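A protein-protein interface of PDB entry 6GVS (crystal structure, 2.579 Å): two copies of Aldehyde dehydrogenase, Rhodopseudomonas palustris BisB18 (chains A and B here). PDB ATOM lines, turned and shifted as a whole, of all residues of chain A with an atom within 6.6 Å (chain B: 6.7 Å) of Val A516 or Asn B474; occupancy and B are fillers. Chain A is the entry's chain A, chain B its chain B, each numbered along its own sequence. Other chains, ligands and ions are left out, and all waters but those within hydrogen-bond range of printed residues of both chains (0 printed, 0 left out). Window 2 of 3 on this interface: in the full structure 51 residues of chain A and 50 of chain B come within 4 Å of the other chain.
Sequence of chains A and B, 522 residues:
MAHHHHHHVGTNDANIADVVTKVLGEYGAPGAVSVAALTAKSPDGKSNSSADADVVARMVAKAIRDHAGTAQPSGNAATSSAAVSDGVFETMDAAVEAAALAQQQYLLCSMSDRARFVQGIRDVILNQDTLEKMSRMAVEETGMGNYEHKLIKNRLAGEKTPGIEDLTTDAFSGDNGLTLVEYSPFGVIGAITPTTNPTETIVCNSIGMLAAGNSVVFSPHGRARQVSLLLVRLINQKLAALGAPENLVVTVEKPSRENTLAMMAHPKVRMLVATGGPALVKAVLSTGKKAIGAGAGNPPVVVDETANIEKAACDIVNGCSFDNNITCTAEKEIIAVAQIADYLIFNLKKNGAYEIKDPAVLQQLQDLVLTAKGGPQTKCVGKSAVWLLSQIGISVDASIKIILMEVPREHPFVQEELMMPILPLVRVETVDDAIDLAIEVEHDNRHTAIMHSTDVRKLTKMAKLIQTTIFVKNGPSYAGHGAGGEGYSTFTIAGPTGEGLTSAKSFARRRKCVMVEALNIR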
ATOM      1  N   ASP A 175     -29.663 -25.936   3.725  1.00  0.00           N
ATOM      2  CA  ASP A 175     -29.152 -25.451   2.449  1.00  0.00           C
ATOM      3  C   ASP A 175     -27.632 -25.373   2.439  1.00  0.00           C
ATOM      4  O   ASP A 175     -27.009 -25.548   1.385  1.00  0.00           O
ATOM      5  CB  ASP A 175     -29.740 -24.077   2.138  1.00  0.00           C
ATOM      6  CG  ASP A 175     -31.251 -24.088   2.092  1.00  0.00           C
ATOM      7  OD1 ASP A 175     -31.825 -25.147   1.760  1.00  0.00           O
ATOM      8  OD2 ASP A 175     -31.863 -23.038   2.385  1.00  0.00           O
ATOM      9  N   ASN A 176     -27.018 -25.105   3.587  1.00  0.00           N
ATOM     10  CA  ASN A 176     -25.571 -24.956   3.663  1.00  0.00           C
ATOM     11  C   ASN A 176     -24.842 -26.285   3.805  1.00  0.00           C
ATOM     12  O   ASN A 176     -23.627 -26.283   4.034  1.00  0.00           O
ATOM     13  CB  ASN A 176     -25.206 -24.036   4.829  1.00  0.00           C
ATOM     14  CG  ASN A 176     -25.693 -22.618   4.621  1.00  0.00           C
ATOM     15  OD1 ASN A 176     -25.588 -22.071   3.524  1.00  0.00           O
ATOM     16  ND2 ASN A 176     -26.238 -22.015   5.674  1.00  0.00           N
ATOM     17  N   GLY A 177     -25.544 -27.406   3.672  1.00  0.00           N
ATOM     18  CA  GLY A 177     -24.915 -28.709   3.741  1.00  0.00           C
ATOM     19  C   GLY A 177     -25.309 -29.505   4.966  1.00  0.00           C
ATOM     20  O   GLY A 177     -26.449 -29.426   5.435  1.00  0.00           O
ATOM     21  N   LEU A 178     -24.369 -30.283   5.492  1.00  0.00           N
ATOM     22  CA  LEU A 178     -24.590 -31.094   6.678  1.00  0.00           C
ATOM     23  C   LEU A 178     -23.555 -30.751   7.736  1.00  0.00           C
ATOM     24  O   LEU A 178     -22.395 -30.471   7.420  1.00  0.00           O
ATOM     25  CB  LEU A 178     -24.520 -32.585   6.349  1.00  0.00           C
ATOM     26  CG  LEU A 178     -24.621 -33.538   7.539  1.00  0.00           C
ATOM     27  CD1 LEU A 178     -25.939 -33.361   8.266  1.00  0.00           C
ATOM     28  CD2 LEU A 178     -24.456 -34.974   7.069  1.00  0.00           C
ATOM     29  N   VAL A 514     -18.293 -29.914   9.279  1.00  0.00           N
ATOM     30  CA  VAL A 514     -19.178 -29.166   8.389  1.00  0.00           C
ATOM     31  C   VAL A 514     -18.867 -29.552   6.947  1.00  0.00           C
ATOM     32  O   VAL A 514     -17.788 -29.245   6.424  1.00  0.00           O
ATOM     33  CB  VAL A 514     -19.041 -27.651   8.596  1.00  0.00           C
ATOM     34  CG1 VAL A 514     -20.065 -26.905   7.762  1.00  0.00           C
ATOM     35  CG2 VAL A 514     -19.198 -27.302  10.068  1.00  0.00           C
ATOM     36  N   MET A 515     -19.807 -30.197   6.308  1.00  0.00           N
ATOM     37  CA  MET A 515     -19.685 -30.565   4.938  1.00  0.00           C
ATOM     38  C   MET A 515     -20.555 -29.571   4.226  1.00  0.00           C
ATOM     39  O   MET A 515     -21.733 -29.646   4.249  1.00  0.00           O
ATOM     40  CB  MET A 515     -20.212 -31.957   4.760  1.00  0.00           C
ATOM     41  CG  MET A 515     -20.337 -32.406   3.345  1.00  0.00           C
ATOM     42  SD  MET A 515     -18.803 -32.896   2.634  1.00  0.00           S
ATOM     43  CE  MET A 515     -18.643 -34.523   3.249  1.00  0.00           C
ATOM     44  N   VAL A 516     -19.914 -28.658   3.549  1.00  0.00           N
ATOM     45  CA  VAL A 516     -20.555 -27.573   2.886  1.00  0.00           C
ATOM     46  C   VAL A 516     -21.231 -27.882   1.581  1.00  0.00           C
ATOM     47  O   VAL A 516     -20.660 -28.448   0.718  1.00  0.00           O
ATOM     48  CB  VAL A 516     -19.496 -26.539   2.644  1.00  0.00           C
ATOM     49  CG1 VAL A 516     -20.048 -25.371   1.929  1.00  0.00           C
ATOM     50  CG2 VAL A 516     -18.924 -26.103   3.942  1.00  0.00           C
ATOM     51  N   GLU A 517     -22.479 -27.503   1.473  1.00  0.00           N
ATOM     52  CA  GLU A 517     -23.262 -27.695   0.281  1.00  0.00           C
ATOM     53  C   GLU A 517     -23.244 -29.100  -0.243  1.00  0.00           C
ATOM     54  O   GLU A 517     -23.022 -29.329  -1.380  1.00  0.00           O
ATOM     55  CB  GLU A 517     -22.883 -26.676  -0.778  1.00  0.00           C
ATOM     56  CG  GLU A 517     -23.266 -25.258  -0.438  1.00  0.00           C
ATOM     57  CD  GLU A 517     -22.840 -24.264  -1.491  1.00  0.00           C
ATOM     58  OE1 GLU A 517     -22.569 -24.652  -2.626  1.00  0.00           O
ATOM     59  OE2 GLU A 517     -22.778 -23.070  -1.193  1.00  0.00           O
ATOM     60  N   ALA A 518     -23.490 -30.048   0.616  1.00  0.00           N
ATOM     61  CA  ALA A 518     -23.449 -31.458   0.254  1.00  0.00           C
ATOM     62  C   ALA A 518     -23.978 -32.278   1.421  1.00  0.00           C
ATOM     63  O   ALA A 518     -23.957 -31.839   2.573  1.00  0.00           O
ATOM     64  CB  ALA A 518     -22.033 -31.905  -0.124  1.00  0.00           C
ATOM     65  N   LEU A 519     -24.457 -33.481   1.099  1.00  0.00           N
ATOM     66  CA  LEU A 519     -25.031 -34.413   2.069  1.00  0.00           C
ATOM     67  C   LEU A 519     -26.286 -33.858   2.737  1.00  0.00           C
ATOM     68  O   LEU A 519     -26.654 -34.288   3.838  1.00  0.00           O
ATOM     69  CB  LEU A 519     -23.996 -34.816   3.125  1.00  0.00           C
ATOM     70  CG  LEU A 519     -22.782 -35.562   2.566  1.00  0.00           C
ATOM     71  CD1 LEU A 519     -21.790 -35.876   3.672  1.00  0.00           C
ATOM     72  CD2 LEU A 519     -23.195 -36.839   1.845  1.00  0.00           C
ATOM     73  N   ALA B 307     -10.180 -32.355  -5.791  1.00  0.00           N
ATOM     74  CA  ALA B 307     -10.878 -31.131  -5.442  1.00  0.00           C
ATOM     75  C   ALA B 307     -11.290 -30.349  -6.683  1.00  0.00           C
ATOM     76  O   ALA B 307     -10.664 -30.438  -7.744  1.00  0.00           O
ATOM     77  CB  ALA B 307      -9.999 -30.244  -4.557  1.00  0.00           C
ATOM     78  N   ASN B 308     -12.378 -29.593  -6.538  1.00  0.00           N
ATOM     79  CA  ASN B 308     -12.727 -28.540  -7.482  1.00  0.00           C
ATOM     80  C   ASN B 308     -11.772 -27.374  -7.258  1.00  0.00           C
ATOM     81  O   ASN B 308     -11.897 -26.644  -6.270  1.00  0.00           O
ATOM     82  CB  ASN B 308     -14.183 -28.129  -7.280  1.00  0.00           C
ATOM     83  CG  ASN B 308     -14.645 -27.094  -8.281  1.00  0.00           C
ATOM     84  OD1 ASN B 308     -13.856 -26.285  -8.775  1.00  0.00           O
ATOM     85  ND2 ASN B 308     -15.940 -27.104  -8.575  1.00  0.00           N
ATOM     86  N   LYS B 311     -12.975 -23.536  -7.454  1.00  0.00           N
ATOM     87  CA  LYS B 311     -13.861 -23.299  -6.320  1.00  0.00           C
ATOM     88  C   LYS B 311     -13.064 -23.244  -5.022  1.00  0.00           C
ATOM     89  O   LYS B 311     -13.257 -22.344  -4.197  1.00  0.00           O
ATOM     90  CB  LYS B 311     -14.938 -24.381  -6.240  1.00  0.00           C
ATOM     91  CG  LYS B 311     -15.988 -24.099  -5.169  1.00  0.00           C
ATOM     92  CD  LYS B 311     -17.077 -25.163  -5.119  1.00  0.00           C
ATOM     93  CE  LYS B 311     -18.226 -24.724  -4.212  1.00  0.00           C
ATOM     94  NZ  LYS B 311     -17.764 -24.365  -2.834  1.00  0.00           N
ATOM     95  N   ALA B 312     -12.155 -24.203  -4.829  1.00  0.00           N
ATOM     96  CA  ALA B 312     -11.307 -24.192  -3.644  1.00  0.00           C
ATOM     97  C   ALA B 312     -10.441 -22.943  -3.591  1.00  0.00           C
ATOM     98  O   ALA B 312     -10.157 -22.432  -2.502  1.00  0.00           O
ATOM     99  CB  ALA B 312     -10.432 -25.446  -3.613  1.00  0.00           C
ATOM    100  N   ASP B 315     -12.775 -20.142  -2.224  1.00  0.00           N
ATOM    101  CA  ASP B 315     -13.068 -20.343  -0.809  1.00  0.00           C
ATOM    102  C   ASP B 315     -11.850 -20.040   0.054  1.00  0.00           C
ATOM    103  O   ASP B 315     -11.963 -19.370   1.087  1.00  0.00           O
ATOM    104  CB  ASP B 315     -13.554 -21.775  -0.577  1.00  0.00           C
ATOM    105  CG  ASP B 315     -14.922 -22.033  -1.185  1.00  0.00           C
ATOM    106  OD1 ASP B 315     -15.539 -21.073  -1.696  1.00  0.00           O
ATOM    107  OD2 ASP B 315     -15.382 -23.194  -1.150  1.00  0.00           O
ATOM    108  N   ILE B 450      -9.254 -27.320   7.497  1.00  0.00           N
ATOM    109  CA  ILE B 450     -10.088 -27.285   6.303  1.00  0.00           C
ATOM    110  C   ILE B 450      -9.523 -28.259   5.277  1.00  0.00           C
ATOM    111  O   ILE B 450      -8.308 -28.462   5.188  1.00  0.00           O
ATOM    112  CB  ILE B 450     -10.173 -25.864   5.701  1.00  0.00           C
ATOM    113  CG1 ILE B 450     -10.672 -24.858   6.741  1.00  0.00           C
ATOM    114  CG2 ILE B 450     -11.090 -25.847   4.489  1.00  0.00           C
ATOM    115  CD1 ILE B 450      -9.589 -24.337   7.666  1.00  0.00           C
ATOM    116  N   MET B 451     -10.418 -28.864   4.497  1.00  0.00           N
ATOM    117  CA  MET B 451     -10.014 -29.735   3.403  1.00  0.00           C
ATOM    118  C   MET B 451     -10.902 -29.487   2.192  1.00  0.00           C
ATOM    119  O   MET B 451     -12.106 -29.248   2.330  1.00  0.00           O
ATOM    120  CB  MET B 451     -10.094 -31.217   3.798  1.00  0.00           C
ATOM    121  CG  MET B 451      -9.372 -32.143   2.825  1.00  0.00           C
ATOM    122  SD  MET B 451      -9.723 -33.892   3.084  1.00  0.00           S
ATOM    123  CE  MET B 451      -8.432 -34.633   2.087  1.00  0.00           C
ATOM    124  N   HIS B 452     -10.300 -29.546   1.007  1.00  0.00           N
ATOM    125  CA  HIS B 452     -11.027 -29.499  -0.258  1.00  0.00           C
ATOM    126  C   HIS B 452     -10.786 -30.810  -0.993  1.00  0.00           C
ATOM    127  O   HIS B 452      -9.640 -31.144  -1.316  1.00  0.00           O
ATOM    128  CB  HIS B 452     -10.592 -28.308  -1.107  1.00  0.00           C
ATOM    129  CG  HIS B 452     -10.984 -26.990  -0.522  1.00  0.00           C
ATOM    130  ND1 HIS B 452     -12.255 -26.471  -0.641  1.00  0.00           N
ATOM    131  CD2 HIS B 452     -10.279 -26.092   0.205  1.00  0.00           C
ATOM    132  CE1 HIS B 452     -12.314 -25.307  -0.022  1.00  0.00           C
ATOM    133  NE2 HIS B 452     -11.127 -25.054   0.500  1.00  0.00           N
ATOM    134  N   SER B 453     -11.863 -31.546  -1.243  1.00  0.00           N
ATOM    135  CA  SER B 453     -11.796 -32.863  -1.855  1.00  0.00           C
ATOM    136  C   SER B 453     -13.216 -33.338  -2.107  1.00  0.00           C
ATOM    137  O   SER B 453     -14.138 -32.993  -1.360  1.00  0.00           O
ATOM    138  CB  SER B 453     -11.048 -33.862  -0.962  1.00  0.00           C
ATOM    139  OG  SER B 453     -11.184 -35.193  -1.434  1.00  0.00           O
ATOM    140  N   THR B 454     -13.386 -34.118  -3.171  1.00  0.00           N
ATOM    141  CA  THR B 454     -14.671 -34.731  -3.468  1.00  0.00           C
ATOM    142  C   THR B 454     -14.722 -36.204  -3.089  1.00  0.00           C
ATOM    143  O   THR B 454     -15.821 -36.758  -2.970  1.00  0.00           O
ATOM    144  CB  THR B 454     -15.006 -34.575  -4.960  1.00  0.00           C
ATOM    145  OG1 THR B 454     -13.984 -35.176  -5.764  1.00  0.00           O
ATOM    146  CG2 THR B 454     -15.118 -33.101  -5.319  1.00  0.00           C
ATOM    147  N   ASP B 455     -13.571 -36.839  -2.885  1.00  0.00           N
ATOM    148  CA  ASP B 455     -13.523 -38.238  -2.476  1.00  0.00           C
ATOM    149  C   ASP B 455     -13.986 -38.345  -1.028  1.00  0.00           C
ATOM    150  O   ASP B 455     -13.325 -37.835  -0.117  1.00  0.00           O
ATOM    151  CB  ASP B 455     -12.111 -38.790  -2.644  1.00  0.00           C
ATOM    152  CG  ASP B 455     -12.067 -40.308  -2.606  1.00  0.00           C
ATOM    153  OD1 ASP B 455     -12.985 -40.915  -2.010  1.00  0.00           O
ATOM    154  OD2 ASP B 455     -11.116 -40.894  -3.172  1.00  0.00           O
ATOM    155  N   LEU B 459     -12.067 -37.244   2.634  1.00  0.00           N
ATOM    156  CA  LEU B 459     -12.647 -36.313   3.595  1.00  0.00           C
ATOM    157  C   LEU B 459     -12.786 -36.972   4.960  1.00  0.00           C
ATOM    158  O   LEU B 459     -12.434 -36.376   5.985  1.00  0.00           O
ATOM    159  CB  LEU B 459     -14.004 -35.824   3.092  1.00  0.00           C
ATOM    160  CG  LEU B 459     -14.010 -34.986   1.813  1.00  0.00           C
ATOM    161  CD1 LEU B 459     -15.431 -34.814   1.296  1.00  0.00           C
ATOM    162  CD2 LEU B 459     -13.373 -33.628   2.049  1.00  0.00           C
ATOM    163  N   VAL B 472     -13.946 -28.083   8.390  1.00  0.00           N
ATOM    164  CA  VAL B 472     -14.753 -27.614   7.270  1.00  0.00           C
ATOM    165  C   VAL B 472     -14.321 -28.351   6.010  1.00  0.00           C
ATOM    166  O   VAL B 472     -13.123 -28.496   5.739  1.00  0.00           O
ATOM    167  CB  VAL B 472     -14.633 -26.089   7.079  1.00  0.00           C
ATOM    168  CG1 VAL B 472     -15.427 -25.646   5.858  1.00  0.00           C
ATOM    169  CG2 VAL B 472     -15.114 -25.355   8.323  1.00  0.00           C
ATOM    170  N   LYS B 473     -15.303 -28.806   5.236  1.00  0.00           N
ATOM    171  CA  LYS B 473     -15.060 -29.547   4.004  1.00  0.00           C
ATOM    172  C   LYS B 473     -15.632 -28.776   2.821  1.00  0.00           C
ATOM    173  O   LYS B 473     -16.832 -28.486   2.783  1.00  0.00           O
ATOM    174  CB  LYS B 473     -15.678 -30.947   4.086  1.00  0.00           C
ATOM    175  CG  LYS B 473     -14.937 -31.889   5.030  1.00  0.00           C
ATOM    176  CD  LYS B 473     -15.781 -33.100   5.438  1.00  0.00           C
ATOM    177  CE  LYS B 473     -16.863 -32.708   6.440  1.00  0.00           C
ATOM    178  NZ  LYS B 473     -17.496 -33.883   7.114  1.00  0.00           N
ATOM    179  N   ASN B 474     -14.766 -28.441   1.865  1.00  0.00           N
ATOM    180  CA  ASN B 474     -15.177 -27.897   0.567  1.00  0.00           C
ATOM    181  C   ASN B 474     -15.882 -26.551   0.709  1.00  0.00           C
ATOM    182  O   ASN B 474     -16.841 -26.254  -0.006  1.00  0.00           O
ATOM    183  CB  ASN B 474     -16.066 -28.893  -0.183  1.00  0.00           C
ATOM    184  CG  ASN B 474     -15.313 -30.131  -0.619  1.00  0.00           C
ATOM    185  OD1 ASN B 474     -14.131 -30.069  -0.961  1.00  0.00           O
ATOM    186  ND2 ASN B 474     -15.994 -31.268  -0.606  1.00  0.00           N
ATOM    187  N   GLY B 475     -15.388 -25.722   1.622  1.00  0.00           N
ATOM    188  CA  GLY B 475     -15.919 -24.396   1.814  1.00  0.00           C
ATOM    189  C   GLY B 475     -14.919 -23.489   2.494  1.00  0.00           C
ATOM    190  O   GLY B 475     -13.817 -23.908   2.864  1.00  0.00           O
ATOM    191  N   PRO B 476     -15.277 -22.218   2.664  1.00  0.00           N
ATOM    192  CA  PRO B 476     -14.404 -21.311   3.415  1.00  0.00           C
ATOM    193  C   PRO B 476     -14.431 -21.638   4.900  1.00  0.00           C
ATOM    194  O   PRO B 476     -15.419 -22.153   5.432  1.00  0.00           O
ATOM    195  CB  PRO B 476     -14.996 -19.926   3.128  1.00  0.00           C
ATOM    196  CG  PRO B 476     -16.436 -20.193   2.828  1.00  0.00           C
ATOM    197  CD  PRO B 476     -16.488 -21.545   2.160  1.00  0.00           C
ATOM    198  N   ALA B 479     -17.260 -20.945   7.285  1.00  0.00           N
ATOM    199  CA  ALA B 479     -18.481 -21.743   7.241  1.00  0.00           C
ATOM    200  C   ALA B 479     -18.695 -22.503   8.545  1.00  0.00           C
ATOM    201  O   ALA B 479     -19.838 -22.805   8.907  1.00  0.00           O
ATOM    202  CB  ALA B 479     -18.430 -22.713   6.060  1.00  0.00           C
ATOM    203  N   GLY B 480     -17.617 -22.822   9.260  1.00  0.00           N
ATOM    204  CA  GLY B 480     -17.733 -23.476  10.551  1.00  0.00           C
ATOM    205  C   GLY B 480     -18.197 -22.575  11.675  1.00  0.00           C
ATOM    206  O   GLY B 480     -18.536 -23.080  12.752  1.00  0.00           O
ATOM    207  N   GLY B 484     -22.458 -19.552   6.251  1.00  0.00           N
ATOM    208  CA  GLY B 484     -22.282 -20.428   5.114  1.00  0.00           C
ATOM    209  C   GLY B 484     -22.316 -21.901   5.446  1.00  0.00           C
ATOM    210  O   GLY B 484     -22.245 -22.729   4.528  1.00  0.00           O
ATOM    211  N   GLY B 485     -22.416 -22.254   6.733  1.00  0.00           N
ATOM    212  CA  GLY B 485     -22.538 -23.633   7.143  1.00  0.00           C
ATOM    213  C   GLY B 485     -23.683 -23.797   8.128  1.00  0.00           C
ATOM    214  O   GLY B 485     -24.264 -22.822   8.608  1.00  0.00           O
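The backbone carbonyl oxygen (O) of Ala B479 sits close to the backbone NH (N) of Gly B485.
The backbone NH of Met B451 is in hydrogen-bond range of the backbone carbonyl oxygen of Val B472 (3.0 Å).
The backbone NH (N) of Met A515 sits at hydrogen-bond distance from the backbone carbonyl oxygen (O) of Leu A178, 2.8 Å away.
The backbone NH of Asn B474 is in hydrogen-bond range of the backbone carbonyl oxygen of Met B451, 2.8 Å away.
The backbone NH (N) of Glu A517 is in hydrogen-bond range of the backbone carbonyl oxygen (O) of Asn A176 (3.1 Å).
O of Ser B453 lies within hydrogen-bond range of ND2 of Asn B474 (2.6 Å).
No position is printed for both chains.
Of the 8 pairs that touch across the chains among the printed residues, none has its exchanged pair printed and touching as well.
CB of Asn A176 touches O of Gly B484, 3.3 Å away.
Gly B485 touches Asn A176.
Val A514 touches Val B472.
CE of Met A515 touches CD1 of Leu B459 (3.8 Å).
Lys B473 touches Met A515 (CE to CB, 3.8 Å).
Asn B474 touches Val A516.
N of Val A516 lies within hydrogen-bond range of O of Lys B473, 3.2 Å away.
N of Lys B473 sits at hydrogen-bond distance from O of Val A514 (2.8 Å).
Hydrophobic or aromatic side chains of chain A that line the printed part of chain B: Met A515 and Val A516.
Of the 21 printed residues of chain B, 6 touch a printed residue of chain A.
Hydrophobic or aromatic side chains of chain B that line the printed part of chain A: Leu B459.
Of chain A, only Val A516 comes within 4 Å of Asn B474.
Printed residues of chain A within 4 Å of Gly B484: Asn A176 (3.3 Å).
Of the printed residues of chain A, Leu B459 touches Met A515.
Of the printed residues of chain A, Val B472 touches Val A514.
Of the printed residues of chain B, Asn A176 touches Gly B484 and Gly B485.
Of the printed residues of chain B, Val A514 touches Val B472 and Lys B473.
Asp A175 touches none of the printed residues of chain B.
His B452 touches none of the printed residues of chain A.
The nearest residue of chain A that does not touch Asn B474 is Met A515 (4.6 Å).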
